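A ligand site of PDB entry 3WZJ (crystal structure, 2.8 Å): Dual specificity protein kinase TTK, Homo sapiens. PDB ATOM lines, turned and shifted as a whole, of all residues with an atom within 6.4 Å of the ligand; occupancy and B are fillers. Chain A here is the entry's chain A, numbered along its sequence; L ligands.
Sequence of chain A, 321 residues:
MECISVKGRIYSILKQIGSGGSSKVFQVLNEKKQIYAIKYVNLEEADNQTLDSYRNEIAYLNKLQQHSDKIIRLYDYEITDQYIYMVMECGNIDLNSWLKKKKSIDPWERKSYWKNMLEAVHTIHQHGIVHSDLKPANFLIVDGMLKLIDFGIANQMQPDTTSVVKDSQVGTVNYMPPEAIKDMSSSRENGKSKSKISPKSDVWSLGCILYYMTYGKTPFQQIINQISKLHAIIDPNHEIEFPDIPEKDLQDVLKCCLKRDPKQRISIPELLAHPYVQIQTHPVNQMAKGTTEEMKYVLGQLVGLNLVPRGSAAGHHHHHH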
ATOM      1  N   LYS A  15     -29.214 -20.359  15.520  1.00  0.00           N
ATOM      2  CA  LYS A  15     -29.258 -18.899  15.344  1.00  0.00           C
ATOM      3  C   LYS A  15     -30.122 -18.487  14.141  1.00  0.00           C
ATOM      4  O   LYS A  15     -30.611 -19.334  13.399  1.00  0.00           O
ATOM      5  CB  LYS A  15     -27.837 -18.328  15.229  1.00  0.00           C
ATOM      6  CG  LYS A  15     -27.715 -16.824  15.465  1.00  0.00           C
ATOM      7  N   ILE A  17     -29.364 -16.441  10.925  1.00  0.00           N
ATOM      8  CA  ILE A  17     -28.243 -15.931  10.120  1.00  0.00           C
ATOM      9  C   ILE A  17     -28.586 -14.642   9.399  1.00  0.00           C
ATOM     10  O   ILE A  17     -27.794 -13.677   9.389  1.00  0.00           O
ATOM     11  CB  ILE A  17     -27.835 -16.977   9.070  1.00  0.00           C
ATOM     12  CG1 ILE A  17     -26.996 -18.084   9.709  1.00  0.00           C
ATOM     13  CG2 ILE A  17     -27.090 -16.331   7.919  1.00  0.00           C
ATOM     14  CD1 ILE A  17     -26.773 -19.258   8.785  1.00  0.00           C
ATOM     15  N   GLY A  18     -29.761 -14.621   8.782  1.00  0.00           N
ATOM     16  CA  GLY A  18     -30.178 -13.514   7.947  1.00  0.00           C
ATOM     17  C   GLY A  18     -31.667 -13.549   7.712  1.00  0.00           C
ATOM     18  O   GLY A  18     -32.344 -14.527   8.060  1.00  0.00           O
ATOM     19  N   SER A  19     -32.174 -12.494   7.092  1.00  0.00           N
ATOM     20  CA  SER A  19     -33.603 -12.283   6.956  1.00  0.00           C
ATOM     21  C   SER A  19     -33.902 -11.617   5.618  1.00  0.00           C
ATOM     22  O   SER A  19     -33.113 -10.803   5.124  1.00  0.00           O
ATOM     23  CB  SER A  19     -34.120 -11.408   8.097  1.00  0.00           C
ATOM     24  N   VAL A  25     -33.169 -17.026   7.054  1.00  0.00           N
ATOM     25  CA  VAL A  25     -32.178 -18.118   7.095  1.00  0.00           C
ATOM     26  C   VAL A  25     -31.746 -18.373   8.527  1.00  0.00           C
ATOM     27  O   VAL A  25     -31.326 -17.451   9.246  1.00  0.00           O
ATOM     28  CB  VAL A  25     -30.941 -17.884   6.194  1.00  0.00           C
ATOM     29  CG1 VAL A  25     -29.959 -19.017   6.343  1.00  0.00           C
ATOM     30  CG2 VAL A  25     -31.338 -17.798   4.743  1.00  0.00           C
ATOM     31  N   GLN A  27     -29.225 -20.814  10.944  1.00  0.00           N
ATOM     32  CA  GLN A  27     -28.272 -21.872  11.228  1.00  0.00           C
ATOM     33  C   GLN A  27     -29.036 -22.859  12.088  1.00  0.00           C
ATOM     34  O   GLN A  27     -29.793 -22.456  12.978  1.00  0.00           O
ATOM     35  CB  GLN A  27     -27.057 -21.326  11.967  1.00  0.00           C
ATOM     36  CG  GLN A  27     -26.099 -22.398  12.434  1.00  0.00           C
ATOM     37  CD  GLN A  27     -24.818 -21.797  12.943  1.00  0.00           C
ATOM     38  OE1 GLN A  27     -24.138 -21.062  12.226  1.00  0.00           O
ATOM     39  NE2 GLN A  27     -24.459 -22.099  14.194  1.00  0.00           N
ATOM     40  N   ILE A  35     -24.491 -29.447  11.639  1.00  0.00           N
ATOM     41  CA  ILE A  35     -24.901 -28.067  11.395  1.00  0.00           C
ATOM     42  C   ILE A  35     -25.415 -27.860   9.948  1.00  0.00           C
ATOM     43  O   ILE A  35     -24.847 -28.405   8.996  1.00  0.00           O
ATOM     44  CB  ILE A  35     -23.748 -27.108  11.791  1.00  0.00           C
ATOM     45  CG1 ILE A  35     -24.231 -25.662  11.936  1.00  0.00           C
ATOM     46  CG2 ILE A  35     -22.568 -27.259  10.826  1.00  0.00           C
ATOM     47  CD1 ILE A  35     -23.163 -24.720  12.470  1.00  0.00           C
ATOM     48  N   TYR A  36     -26.505 -27.113   9.787  1.00  0.00           N
ATOM     49  CA  TYR A  36     -27.089 -26.840   8.471  1.00  0.00           C
ATOM     50  C   TYR A  36     -27.647 -25.427   8.365  1.00  0.00           C
ATOM     51  O   TYR A  36     -27.689 -24.671   9.349  1.00  0.00           O
ATOM     52  CB  TYR A  36     -28.187 -27.852   8.137  1.00  0.00           C
ATOM     53  CG  TYR A  36     -27.648 -29.203   7.771  1.00  0.00           C
ATOM     54  CD1 TYR A  36     -27.208 -29.467   6.472  1.00  0.00           C
ATOM     55  CD2 TYR A  36     -27.560 -30.212   8.720  1.00  0.00           C
ATOM     56  CE1 TYR A  36     -26.680 -30.702   6.131  1.00  0.00           C
ATOM     57  CE2 TYR A  36     -27.040 -31.459   8.388  1.00  0.00           C
ATOM     58  CZ  TYR A  36     -26.599 -31.694   7.095  1.00  0.00           C
ATOM     59  OH  TYR A  36     -26.087 -32.923   6.778  1.00  0.00           O
ATOM     60  N   ALA A  37     -28.083 -25.071   7.150  1.00  0.00           N
ATOM     61  CA  ALA A  37     -28.714 -23.784   6.900  1.00  0.00           C
ATOM     62  C   ALA A  37     -30.071 -23.971   6.247  1.00  0.00           C
ATOM     63  O   ALA A  37     -30.135 -24.380   5.102  1.00  0.00           O
ATOM     64  CB  ALA A  37     -27.814 -22.907   6.033  1.00  0.00           C
ATOM     65  N   LYS A  39     -33.319 -22.144   4.922  1.00  0.00           N
ATOM     66  CA  LYS A  39     -33.989 -20.916   4.502  1.00  0.00           C
ATOM     67  C   LYS A  39     -35.490 -21.175   4.476  1.00  0.00           C
ATOM     68  O   LYS A  39     -35.953 -22.156   3.899  1.00  0.00           O
ATOM     69  CB  LYS A  39     -33.500 -20.473   3.134  1.00  0.00           C
ATOM     70  CG  LYS A  39     -34.336 -19.427   2.441  1.00  0.00           C
ATOM     71  CD  LYS A  39     -33.481 -18.750   1.399  1.00  0.00           C
ATOM     72  CE  LYS A  39     -34.206 -18.509   0.083  1.00  0.00           C
ATOM     73  NZ  LYS A  39     -33.374 -17.606  -0.765  1.00  0.00           N
ATOM     74  N   GLU A  57     -35.828 -19.971  -8.272  1.00  0.00           N
ATOM     75  CA  GLU A  57     -34.631 -20.093  -7.451  1.00  0.00           C
ATOM     76  C   GLU A  57     -34.335 -21.540  -7.073  1.00  0.00           C
ATOM     77  O   GLU A  57     -33.219 -22.007  -7.256  1.00  0.00           O
ATOM     78  CB  GLU A  57     -34.720 -19.205  -6.204  1.00  0.00           C
ATOM     79  CG  GLU A  57     -33.368 -18.867  -5.594  1.00  0.00           C
ATOM     80  CD  GLU A  57     -33.474 -18.308  -4.179  1.00  0.00           C
ATOM     81  OE1 GLU A  57     -34.153 -18.906  -3.322  1.00  0.00           O
ATOM     82  OE2 GLU A  57     -32.836 -17.267  -3.905  1.00  0.00           O
ATOM     83  N   ILE A  58     -35.339 -22.267  -6.561  1.00  0.00           N
ATOM     84  CA  ILE A  58     -35.111 -23.650  -6.147  1.00  0.00           C
ATOM     85  C   ILE A  58     -34.690 -24.483  -7.354  1.00  0.00           C
ATOM     86  O   ILE A  58     -33.748 -25.245  -7.281  1.00  0.00           O
ATOM     87  CB  ILE A  58     -36.338 -24.312  -5.454  1.00  0.00           C
ATOM     88  CG1 ILE A  58     -37.308 -23.273  -4.908  1.00  0.00           C
ATOM     89  CG2 ILE A  58     -35.875 -25.221  -4.330  1.00  0.00           C
ATOM     90  CD1 ILE A  58     -38.259 -23.781  -3.846  1.00  0.00           C
ATOM     91  N   LEU A  61     -31.032 -23.587  -8.279  1.00  0.00           N
ATOM     92  CA  LEU A  61     -30.133 -24.100  -7.237  1.00  0.00           C
ATOM     93  C   LEU A  61     -30.053 -25.622  -7.318  1.00  0.00           C
ATOM     94  O   LEU A  61     -28.966 -26.199  -7.300  1.00  0.00           O
ATOM     95  CB  LEU A  61     -30.555 -23.638  -5.852  1.00  0.00           C
ATOM     96  CG  LEU A  61     -29.750 -24.190  -4.664  1.00  0.00           C
ATOM     97  CD1 LEU A  61     -28.259 -24.164  -4.908  1.00  0.00           C
ATOM     98  CD2 LEU A  61     -30.110 -23.475  -3.377  1.00  0.00           C
ATOM     99  N   ILE A  72     -23.424 -23.392  -3.432  1.00  0.00           N
ATOM    100  CA  ILE A  72     -23.982 -23.875  -2.172  1.00  0.00           C
ATOM    101  C   ILE A  72     -24.780 -25.174  -2.381  1.00  0.00           C
ATOM    102  O   ILE A  72     -25.627 -25.239  -3.276  1.00  0.00           O
ATOM    103  CB  ILE A  72     -24.856 -22.773  -1.529  1.00  0.00           C
ATOM    104  CG1 ILE A  72     -25.298 -23.162  -0.118  1.00  0.00           C
ATOM    105  CG2 ILE A  72     -26.053 -22.435  -2.412  1.00  0.00           C
ATOM    106  CD1 ILE A  72     -24.206 -23.126   0.941  1.00  0.00           C
ATOM    107  N   MET A  86     -35.739 -24.666   2.512  1.00  0.00           N
ATOM    108  CA  MET A  86     -34.569 -25.092   1.755  1.00  0.00           C
ATOM    109  C   MET A  86     -33.521 -25.571   2.733  1.00  0.00           C
ATOM    110  O   MET A  86     -32.973 -24.761   3.509  1.00  0.00           O
ATOM    111  CB  MET A  86     -34.028 -23.922   0.942  1.00  0.00           C
ATOM    112  CG  MET A  86     -34.342 -23.954  -0.527  1.00  0.00           C
ATOM    113  SD  MET A  86     -34.644 -22.303  -1.166  1.00  0.00           S
ATOM    114  CE  MET A  86     -33.768 -22.414  -2.717  1.00  0.00           C
ATOM    115  N   MET A  88     -29.917 -26.471   3.235  1.00  0.00           N
ATOM    116  CA  MET A  88     -28.654 -26.253   2.522  1.00  0.00           C
ATOM    117  C   MET A  88     -27.457 -26.434   3.436  1.00  0.00           C
ATOM    118  O   MET A  88     -27.603 -26.479   4.659  1.00  0.00           O
ATOM    119  CB  MET A  88     -28.612 -24.843   1.926  1.00  0.00           C
ATOM    120  CG  MET A  88     -29.782 -24.552   1.018  1.00  0.00           C
ATOM    121  SD  MET A  88     -30.162 -22.811   0.962  1.00  0.00           S
ATOM    122  CE  MET A  88     -29.147 -22.352  -0.423  1.00  0.00           C
ATOM    123  N   GLU A  89     -26.279 -26.537   2.854  1.00  0.00           N
ATOM    124  CA  GLU A  89     -25.068 -26.564   3.660  1.00  0.00           C
ATOM    125  C   GLU A  89     -24.845 -25.208   4.345  1.00  0.00           C
ATOM    126  O   GLU A  89     -25.237 -24.147   3.849  1.00  0.00           O
ATOM    127  CB  GLU A  89     -23.840 -27.074   2.865  1.00  0.00           C
ATOM    128  CG  GLU A  89     -22.943 -26.000   2.244  1.00  0.00           C
ATOM    129  CD  GLU A  89     -22.142 -26.522   1.075  1.00  0.00           C
ATOM    130  OE1 GLU A  89     -22.426 -26.106  -0.076  1.00  0.00           O
ATOM    131  OE2 GLU A  89     -21.244 -27.370   1.275  1.00  0.00           O
ATOM    132  N   CYS A  90     -24.208 -25.267   5.506  1.00  0.00           N
ATOM    133  CA  CYS A  90     -23.987 -24.086   6.302  1.00  0.00           C
ATOM    134  C   CYS A  90     -22.530 -23.696   6.176  1.00  0.00           C
ATOM    135  O   CYS A  90     -21.643 -24.543   6.265  1.00  0.00           O
ATOM    136  CB  CYS A  90     -24.344 -24.391   7.755  1.00  0.00           C
ATOM    137  SG  CYS A  90     -24.101 -23.018   8.875  1.00  0.00           S
ATOM    138  N   GLY A  91     -22.307 -22.403   5.978  1.00  0.00           N
ATOM    139  CA  GLY A  91     -20.952 -21.895   5.822  1.00  0.00           C
ATOM    140  C   GLY A  91     -20.321 -21.452   7.122  1.00  0.00           C
ATOM    141  O   GLY A  91     -21.022 -21.025   8.047  1.00  0.00           O
ATOM    142  N   ASN A  92     -19.001 -21.577   7.183  1.00  0.00           N
ATOM    143  CA  ASN A  92     -18.195 -20.985   8.249  1.00  0.00           C
ATOM    144  C   ASN A  92     -18.509 -19.495   8.381  1.00  0.00           C
ATOM    145  O   ASN A  92     -19.083 -19.062   9.386  1.00  0.00           O
ATOM    146  CB  ASN A  92     -16.702 -21.157   7.976  1.00  0.00           C
ATOM    147  CG  ASN A  92     -16.304 -22.609   7.701  1.00  0.00           C
ATOM    148  OD1 ASN A  92     -17.143 -23.468   7.429  1.00  0.00           O
ATOM    149  ND2 ASN A  92     -15.005 -22.881   7.779  1.00  0.00           N
ATOM    150  N   ILE A  93     -18.153 -18.724   7.361  1.00  0.00           N
ATOM    151  CA  ILE A  93     -18.248 -17.265   7.402  1.00  0.00           C
ATOM    152  C   ILE A  93     -18.533 -16.748   5.992  1.00  0.00           C
ATOM    153  O   ILE A  93     -17.961 -17.258   5.014  1.00  0.00           O
ATOM    154  CB  ILE A  93     -16.940 -16.631   7.954  1.00  0.00           C
ATOM    155  CG1 ILE A  93     -16.660 -17.103   9.395  1.00  0.00           C
ATOM    156  CG2 ILE A  93     -17.001 -15.116   7.916  1.00  0.00           C
ATOM    157  CD1 ILE A  93     -15.216 -17.437   9.691  1.00  0.00           C
ATOM    158  N   ASP A  94     -19.433 -15.772   5.869  1.00  0.00           N
ATOM    159  CA  ASP A  94     -19.681 -15.136   4.578  1.00  0.00           C
ATOM    160  C   ASP A  94     -18.526 -14.194   4.275  1.00  0.00           C
ATOM    161  O   ASP A  94     -17.985 -13.582   5.180  1.00  0.00           O
ATOM    162  CB  ASP A  94     -21.020 -14.387   4.559  1.00  0.00           C
ATOM    163  CG  ASP A  94     -20.980 -13.102   5.339  1.00  0.00           C
ATOM    164  OD1 ASP A  94     -20.797 -12.041   4.709  1.00  0.00           O
ATOM    165  OD2 ASP A  94     -21.122 -13.150   6.581  1.00  0.00           O
ATOM    166  N   SER A  97     -18.016 -10.431   5.898  1.00  0.00           N
ATOM    167  CA  SER A  97     -17.550 -10.328   7.269  1.00  0.00           C
ATOM    168  C   SER A  97     -16.104 -10.819   7.431  1.00  0.00           C
ATOM    169  O   SER A  97     -15.375 -10.319   8.287  1.00  0.00           O
ATOM    170  CB  SER A  97     -18.489 -11.061   8.233  1.00  0.00           C
ATOM    171  OG  SER A  97     -18.438 -12.457   8.026  1.00  0.00           O
ATOM    172  N   ALA A 137     -21.050 -10.506   0.057  1.00  0.00           N
ATOM    173  CA  ALA A 137     -22.166 -11.069   0.819  1.00  0.00           C
ATOM    174  C   ALA A 137     -22.853 -12.246   0.093  1.00  0.00           C
ATOM    175  O   ALA A 137     -23.537 -13.054   0.714  1.00  0.00           O
ATOM    176  CB  ALA A 137     -23.182  -9.985   1.134  1.00  0.00           C
ATOM    177  N   ASN A 138     -22.680 -12.304  -1.227  1.00  0.00           N
ATOM    178  CA  ASN A 138     -23.126 -13.426  -2.021  1.00  0.00           C
ATOM    179  C   ASN A 138     -22.190 -14.642  -1.972  1.00  0.00           C
ATOM    180  O   ASN A 138     -22.573 -15.729  -2.418  1.00  0.00           O
ATOM    181  CB  ASN A 138     -23.363 -12.985  -3.455  1.00  0.00           C
ATOM    182  CG  ASN A 138     -24.387 -11.872  -3.559  1.00  0.00           C
ATOM    183  OD1 ASN A 138     -24.152 -10.840  -4.193  1.00  0.00           O
ATOM    184  ND2 ASN A 138     -25.535 -12.081  -2.939  1.00  0.00           N
ATOM    185  N   PHE A 139     -21.001 -14.470  -1.403  1.00  0.00           N
ATOM    186  CA  PHE A 139     -20.040 -15.583  -1.308  1.00  0.00           C
ATOM    187  C   PHE A 139     -19.835 -16.072   0.113  1.00  0.00           C
ATOM    188  O   PHE A 139     -20.213 -15.385   1.077  1.00  0.00           O
ATOM    189  CB  PHE A 139     -18.706 -15.248  -1.991  1.00  0.00           C
ATOM    190  CG  PHE A 139     -18.849 -14.935  -3.448  1.00  0.00           C
ATOM    191  CD1 PHE A 139     -18.859 -15.954  -4.390  1.00  0.00           C
ATOM    192  CD2 PHE A 139     -19.027 -13.628  -3.887  1.00  0.00           C
ATOM    193  CE1 PHE A 139     -19.019 -15.675  -5.725  1.00  0.00           C
ATOM    194  CE2 PHE A 139     -19.177 -13.329  -5.220  1.00  0.00           C
ATOM    195  CZ  PHE A 139     -19.174 -14.352  -6.144  1.00  0.00           C
ATOM    196  N   LEU A 140     -19.221 -17.244   0.244  1.00  0.00           N
ATOM    197  CA  LEU A 140     -19.191 -17.985   1.484  1.00  0.00           C
ATOM    198  C   LEU A 140     -17.995 -18.921   1.516  1.00  0.00           C
ATOM    199  O   LEU A 140     -17.613 -19.483   0.492  1.00  0.00           O
ATOM    200  CB  LEU A 140     -20.452 -18.816   1.580  1.00  0.00           C
ATOM    201  CG  LEU A 140     -20.995 -19.225   2.935  1.00  0.00           C
ATOM    202  CD1 LEU A 140     -22.040 -18.213   3.407  1.00  0.00           C
ATOM    203  CD2 LEU A 140     -21.629 -20.604   2.771  1.00  0.00           C
ATOM    204  N   ILE A 149     -23.842 -18.412  -3.228  1.00  0.00           N
ATOM    205  CA  ILE A 149     -24.965 -18.861  -2.421  1.00  0.00           C
ATOM    206  C   ILE A 149     -26.315 -18.518  -3.025  1.00  0.00           C
ATOM    207  O   ILE A 149     -27.274 -19.285  -2.882  1.00  0.00           O
ATOM    208  CB  ILE A 149     -24.861 -18.404  -0.943  1.00  0.00           C
ATOM    209  CG1 ILE A 149     -24.783 -16.877  -0.829  1.00  0.00           C
ATOM    210  CG2 ILE A 149     -23.662 -19.083  -0.292  1.00  0.00           C
ATOM    211  CD1 ILE A 149     -24.604 -16.354   0.575  1.00  0.00           C
ATOM    212  N   ASP A 150     -26.390 -17.376  -3.712  1.00  0.00           N
ATOM    213  CA  ASP A 150     -27.592 -16.997  -4.442  1.00  0.00           C
ATOM    214  C   ASP A 150     -27.304 -16.587  -5.912  1.00  0.00           C
ATOM    215  O   ASP A 150     -26.143 -16.479  -6.325  1.00  0.00           O
ATOM    216  CB  ASP A 150     -28.354 -15.894  -3.696  1.00  0.00           C
ATOM    217  CG  ASP A 150     -27.787 -14.537  -3.949  1.00  0.00           C
ATOM    218  OD1 ASP A 150     -26.566 -14.364  -3.750  1.00  0.00           O
ATOM    219  OD2 ASP A 150     -28.565 -13.637  -4.360  1.00  0.00           O
ATOM    220  N   PHE A 151     -28.373 -16.344  -6.673  1.00  0.00           N
ATOM    221  CA  PHE A 151     -28.264 -16.124  -8.114  1.00  0.00           C
ATOM    222  C   PHE A 151     -28.814 -14.767  -8.563  1.00  0.00           C
ATOM    223  O   PHE A 151     -28.926 -14.505  -9.756  1.00  0.00           O
ATOM    224  CB  PHE A 151     -28.998 -17.237  -8.859  1.00  0.00           C
ATOM    225  CG  PHE A 151     -28.588 -18.608  -8.447  1.00  0.00           C
ATOM    226  CD1 PHE A 151     -27.435 -19.196  -8.952  1.00  0.00           C
ATOM    227  CD2 PHE A 151     -29.367 -19.337  -7.555  1.00  0.00           C
ATOM    228  CE1 PHE A 151     -27.054 -20.470  -8.567  1.00  0.00           C
ATOM    229  CE2 PHE A 151     -28.996 -20.612  -7.168  1.00  0.00           C
ATOM    230  CZ  PHE A 151     -27.845 -21.178  -7.679  1.00  0.00           C
ATOM    231  N   GLN A 156     -32.765 -10.329  -2.382  1.00  0.00           N
ATOM    232  CA  GLN A 156     -31.558 -10.441  -1.560  1.00  0.00           C
ATOM    233  C   GLN A 156     -31.884 -10.326  -0.064  1.00  0.00           C
ATOM    234  O   GLN A 156     -32.838  -9.644   0.326  1.00  0.00           O
ATOM    235  CB  GLN A 156     -30.551  -9.366  -1.975  1.00  0.00           C
ATOM    236  CG  GLN A 156     -29.086  -9.758  -1.797  1.00  0.00           C
ATOM    237  CD  GLN A 156     -28.388 -10.141  -3.107  1.00  0.00           C
ATOM    238  OE1 GLN A 156     -27.161 -10.029  -3.221  1.00  0.00           O
ATOM    239  NE2 GLN A 156     -29.155 -10.584  -4.100  1.00  0.00           N
ATOM    240  N   MET A 157     -31.080 -10.991   0.760  1.00  0.00           N
ATOM    241  CA  MET A 157     -31.236 -10.969   2.215  1.00  0.00           C
ATOM    242  C   MET A 157     -30.022 -10.305   2.874  1.00  0.00           C
ATOM    243  O   MET A 157     -28.942 -10.266   2.287  1.00  0.00           O
ATOM    244  CB  MET A 157     -31.400 -12.391   2.761  1.00  0.00           C
ATOM    245  CG  MET A 157     -32.724 -13.061   2.444  1.00  0.00           C
ATOM    246  SD  MET A 157     -32.924 -14.624   3.301  1.00  0.00           S
ATOM    247  CE  MET A 157     -31.665 -15.594   2.463  1.00  0.00           C
ATOM    248  N   GLN A 158     -30.202  -9.800   4.096  1.00  0.00           N
ATOM    249  CA  GLN A 158     -29.091  -9.184   4.838  1.00  0.00           C
ATOM    250  C   GLN A 158     -28.938  -9.818   6.220  1.00  0.00           C
ATOM    251  O   GLN A 158     -29.887 -10.412   6.726  1.00  0.00           O
ATOM    252  CB  GLN A 158     -29.279  -7.657   4.942  1.00  0.00           C
ATOM    253  CG  GLN A 158     -30.530  -7.183   5.661  1.00  0.00           C
ATOM    254  CD  GLN A 158     -31.802  -7.273   4.824  1.00  0.00           C
ATOM    255  OE1 GLN A 158     -31.759  -7.579   3.626  1.00  0.00           O
ATOM    256  NE2 GLN A 158     -32.937  -7.016   5.458  1.00  0.00           N
ATOM    257  N   PRO A 159     -27.730  -9.714   6.824  1.00  0.00           N
ATOM    258  CA  PRO A 159     -27.449 -10.343   8.130  1.00  0.00           C
ATOM    259  C   PRO A 159     -28.340  -9.883   9.295  1.00  0.00           C
ATOM    260  O   PRO A 159     -28.981  -8.821   9.211  1.00  0.00           O
ATOM    261  CB  PRO A 159     -25.990  -9.958   8.397  1.00  0.00           C
ATOM    262  CG  PRO A 159     -25.406  -9.734   7.051  1.00  0.00           C
ATOM    263  CD  PRO A 159     -26.509  -9.115   6.245  1.00  0.00           C
HETATM  264  O1  LIG L   1     -30.718 -18.104   0.311  1.00  0.00           O
HETATM  265  C1  LIG L   1     -29.668 -18.664   0.080  1.00  0.00           C
HETATM  266  N1  LIG L   1     -29.374 -19.111  -1.277  1.00  0.00           N
HETATM  267  C2  LIG L   1     -30.397 -18.841  -2.280  1.00  0.00           C
HETATM  268  C3  LIG L   1     -31.399 -19.956  -2.393  1.00  0.00           C
HETATM  269  C4  LIG L   1     -30.382 -19.746  -3.495  1.00  0.00           C
HETATM  270  C5  LIG L   1     -28.634 -18.915   1.199  1.00  0.00           C
HETATM  271  C6  LIG L   1     -27.850 -20.073   1.154  1.00  0.00           C
HETATM  272  C7  LIG L   1     -26.899 -20.323   2.154  1.00  0.00           C
HETATM  273  C8  LIG L   1     -26.769 -19.369   3.173  1.00  0.00           C
HETATM  274  C9  LIG L   1     -27.541 -18.213   3.226  1.00  0.00           C
HETATM  275  C10 LIG L   1     -28.484 -17.980   2.211  1.00  0.00           C
HETATM  276  C11 LIG L   1     -25.736 -19.590   4.288  1.00  0.00           C
HETATM  277  C12 LIG L   1     -25.264 -20.785   4.742  1.00  0.00           C
HETATM  278  N2  LIG L   1     -24.370 -20.512   5.720  1.00  0.00           N
HETATM  279  C13 LIG L   1     -24.303 -19.130   5.849  1.00  0.00           C
HETATM  280  N3  LIG L   1     -25.145 -18.566   4.961  1.00  0.00           N
HETATM  281  N4  LIG L   1     -25.313 -17.183   4.815  1.00  0.00           N
HETATM  282  C14 LIG L   1     -24.594 -16.350   5.634  1.00  0.00           C
HETATM  283  N5  LIG L   1     -24.669 -14.911   5.564  1.00  0.00           N
HETATM  284  C15 LIG L   1     -25.777 -14.056   5.168  1.00  0.00           C
HETATM  285  C16 LIG L   1     -27.049 -14.785   4.788  1.00  0.00           C
HETATM  286  C17 LIG L   1     -28.122 -13.712   4.634  1.00  0.00           C
HETATM  287  C18 LIG L   1     -27.743 -12.601   3.645  1.00  0.00           C
HETATM  288  C19 LIG L   1     -26.311 -12.062   3.749  1.00  0.00           C
HETATM  289  C20 LIG L   1     -25.298 -13.166   4.012  1.00  0.00           C
HETATM  290  C21 LIG L   1     -23.687 -16.900   6.606  1.00  0.00           C
HETATM  291  C22 LIG L   1     -23.546 -18.285   6.715  1.00  0.00           C
HETATM  292  N6  LIG L   1     -22.623 -18.880   7.706  1.00  0.00           N
HETATM  293  C23 LIG L   1     -21.989 -17.957   8.694  1.00  0.00           C
HETATM  294  C24 LIG L   1     -22.711 -17.943  10.061  1.00  0.00           C
HETATM  295  C25 LIG L   1     -22.113 -19.036  10.884  1.00  0.00           C
HETATM  296  C26 LIG L   1     -22.185 -18.862  12.394  1.00  0.00           C
HETATM  297  O2  LIG L   1     -21.894 -17.470  12.793  1.00  0.00           O
HETATM  298  C27 LIG L   1     -22.701 -16.452  12.089  1.00  0.00           C
HETATM  299  C28 LIG L   1     -22.561 -16.565  10.578  1.00  0.00           C
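The backbone carbonyl oxygen (O) of Ile 149 sits at hydrogen-bond distance from a nitrogen (N1) of the ligand, 2.6 Å away. NZ of Lys 39 lies within hydrogen-bond range of O1 of the ligand (2.9 Å). O of Gly 91 is in hydrogen-bond range of N6 of the ligand (2.7 Å). The backbone NH (N) of Gly 91 lies within hydrogen-bond range of a nitrogen (N2) of the ligand.
N of Ile 17 lies within hydrogen-bond range of O of Val 25 (2.8 Å). The side-chain carboxylate (OE1) of Glu 57 is in salt-bridge range of the side-chain amino group (NZ) of Lys 39 (3.0 Å). N of Met 88 sits at hydrogen-bond distance from O of Ala 37 (2.8 Å). The backbone NH (N) of Val 25 lies within hydrogen-bond range of the backbone carbonyl oxygen (O) of Gly 18 (2.8 Å). The side-chain amide nitrogen of Gln 156 lies within hydrogen-bond range of the side-chain carboxylate of Asp 150, at 3.1 Å. The backbone carbonyl oxygen (O) of Asn 138 sits close to the backbone NH (N) of Ile 149, 3.1 Å away. The side-chain hydroxyl (OG) of Ser 97 sits at hydrogen-bond distance from the backbone carbonyl oxygen (O) of Asp 94 (3.1 Å). The side-chain carboxylate (OD1) of Asp 150 sits at hydrogen-bond distance from the side-chain amide nitrogen (ND2) of Asn 138, at 2.6 Å.
CG2 of Ile 17 touches C14 of the ligand, at 3.4 Å. Gly 18 touches the ligand. Val 25 touches the ligand. Gln 27 touches the ligand (OE1 to C26, 2.9 Å). Ala 37 touches the ligand (CB to C12, 3.6 Å). Glu 57 touches the ligand (OE1 to C3, 3.1 Å). Leu 61 touches the ligand. CG1 of Ile 72 touches C7 of the ligand, at 3.97 Å. Met 86 touches the ligand. Met 88 touches the ligand. Glu 89 touches the ligand. Cys 90 touches the ligand. Asn 92 touches the ligand (O to C23, 3.2 Å). CB of Asp 94 touches N5 of the ligand (3.8 Å). Ala 137 touches the ligand. Leu 140 touches the ligand. Asp 150 touches the ligand (CB to C2, 3.9 Å). Met 157 touches the ligand (O to C18, 3.0 Å). Gln 158 touches the ligand. Pro 159 touches the ligand. Hydrophobic or aromatic side chains within 4 Å of the ligand: Ile 17, Val 25, Ala 37, Leu 61, Ile 72, Met 86, Met 88, Leu 140, Met 157 and Pro 159. Of the 34 residues printed, 23 come within 4 Å of the ligand. Along chain A the residues within 4 Å of the ligand span positions 17 to 159. The nearest printed residue that does not touch the ligand is Ile 93 (4.02 Å).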
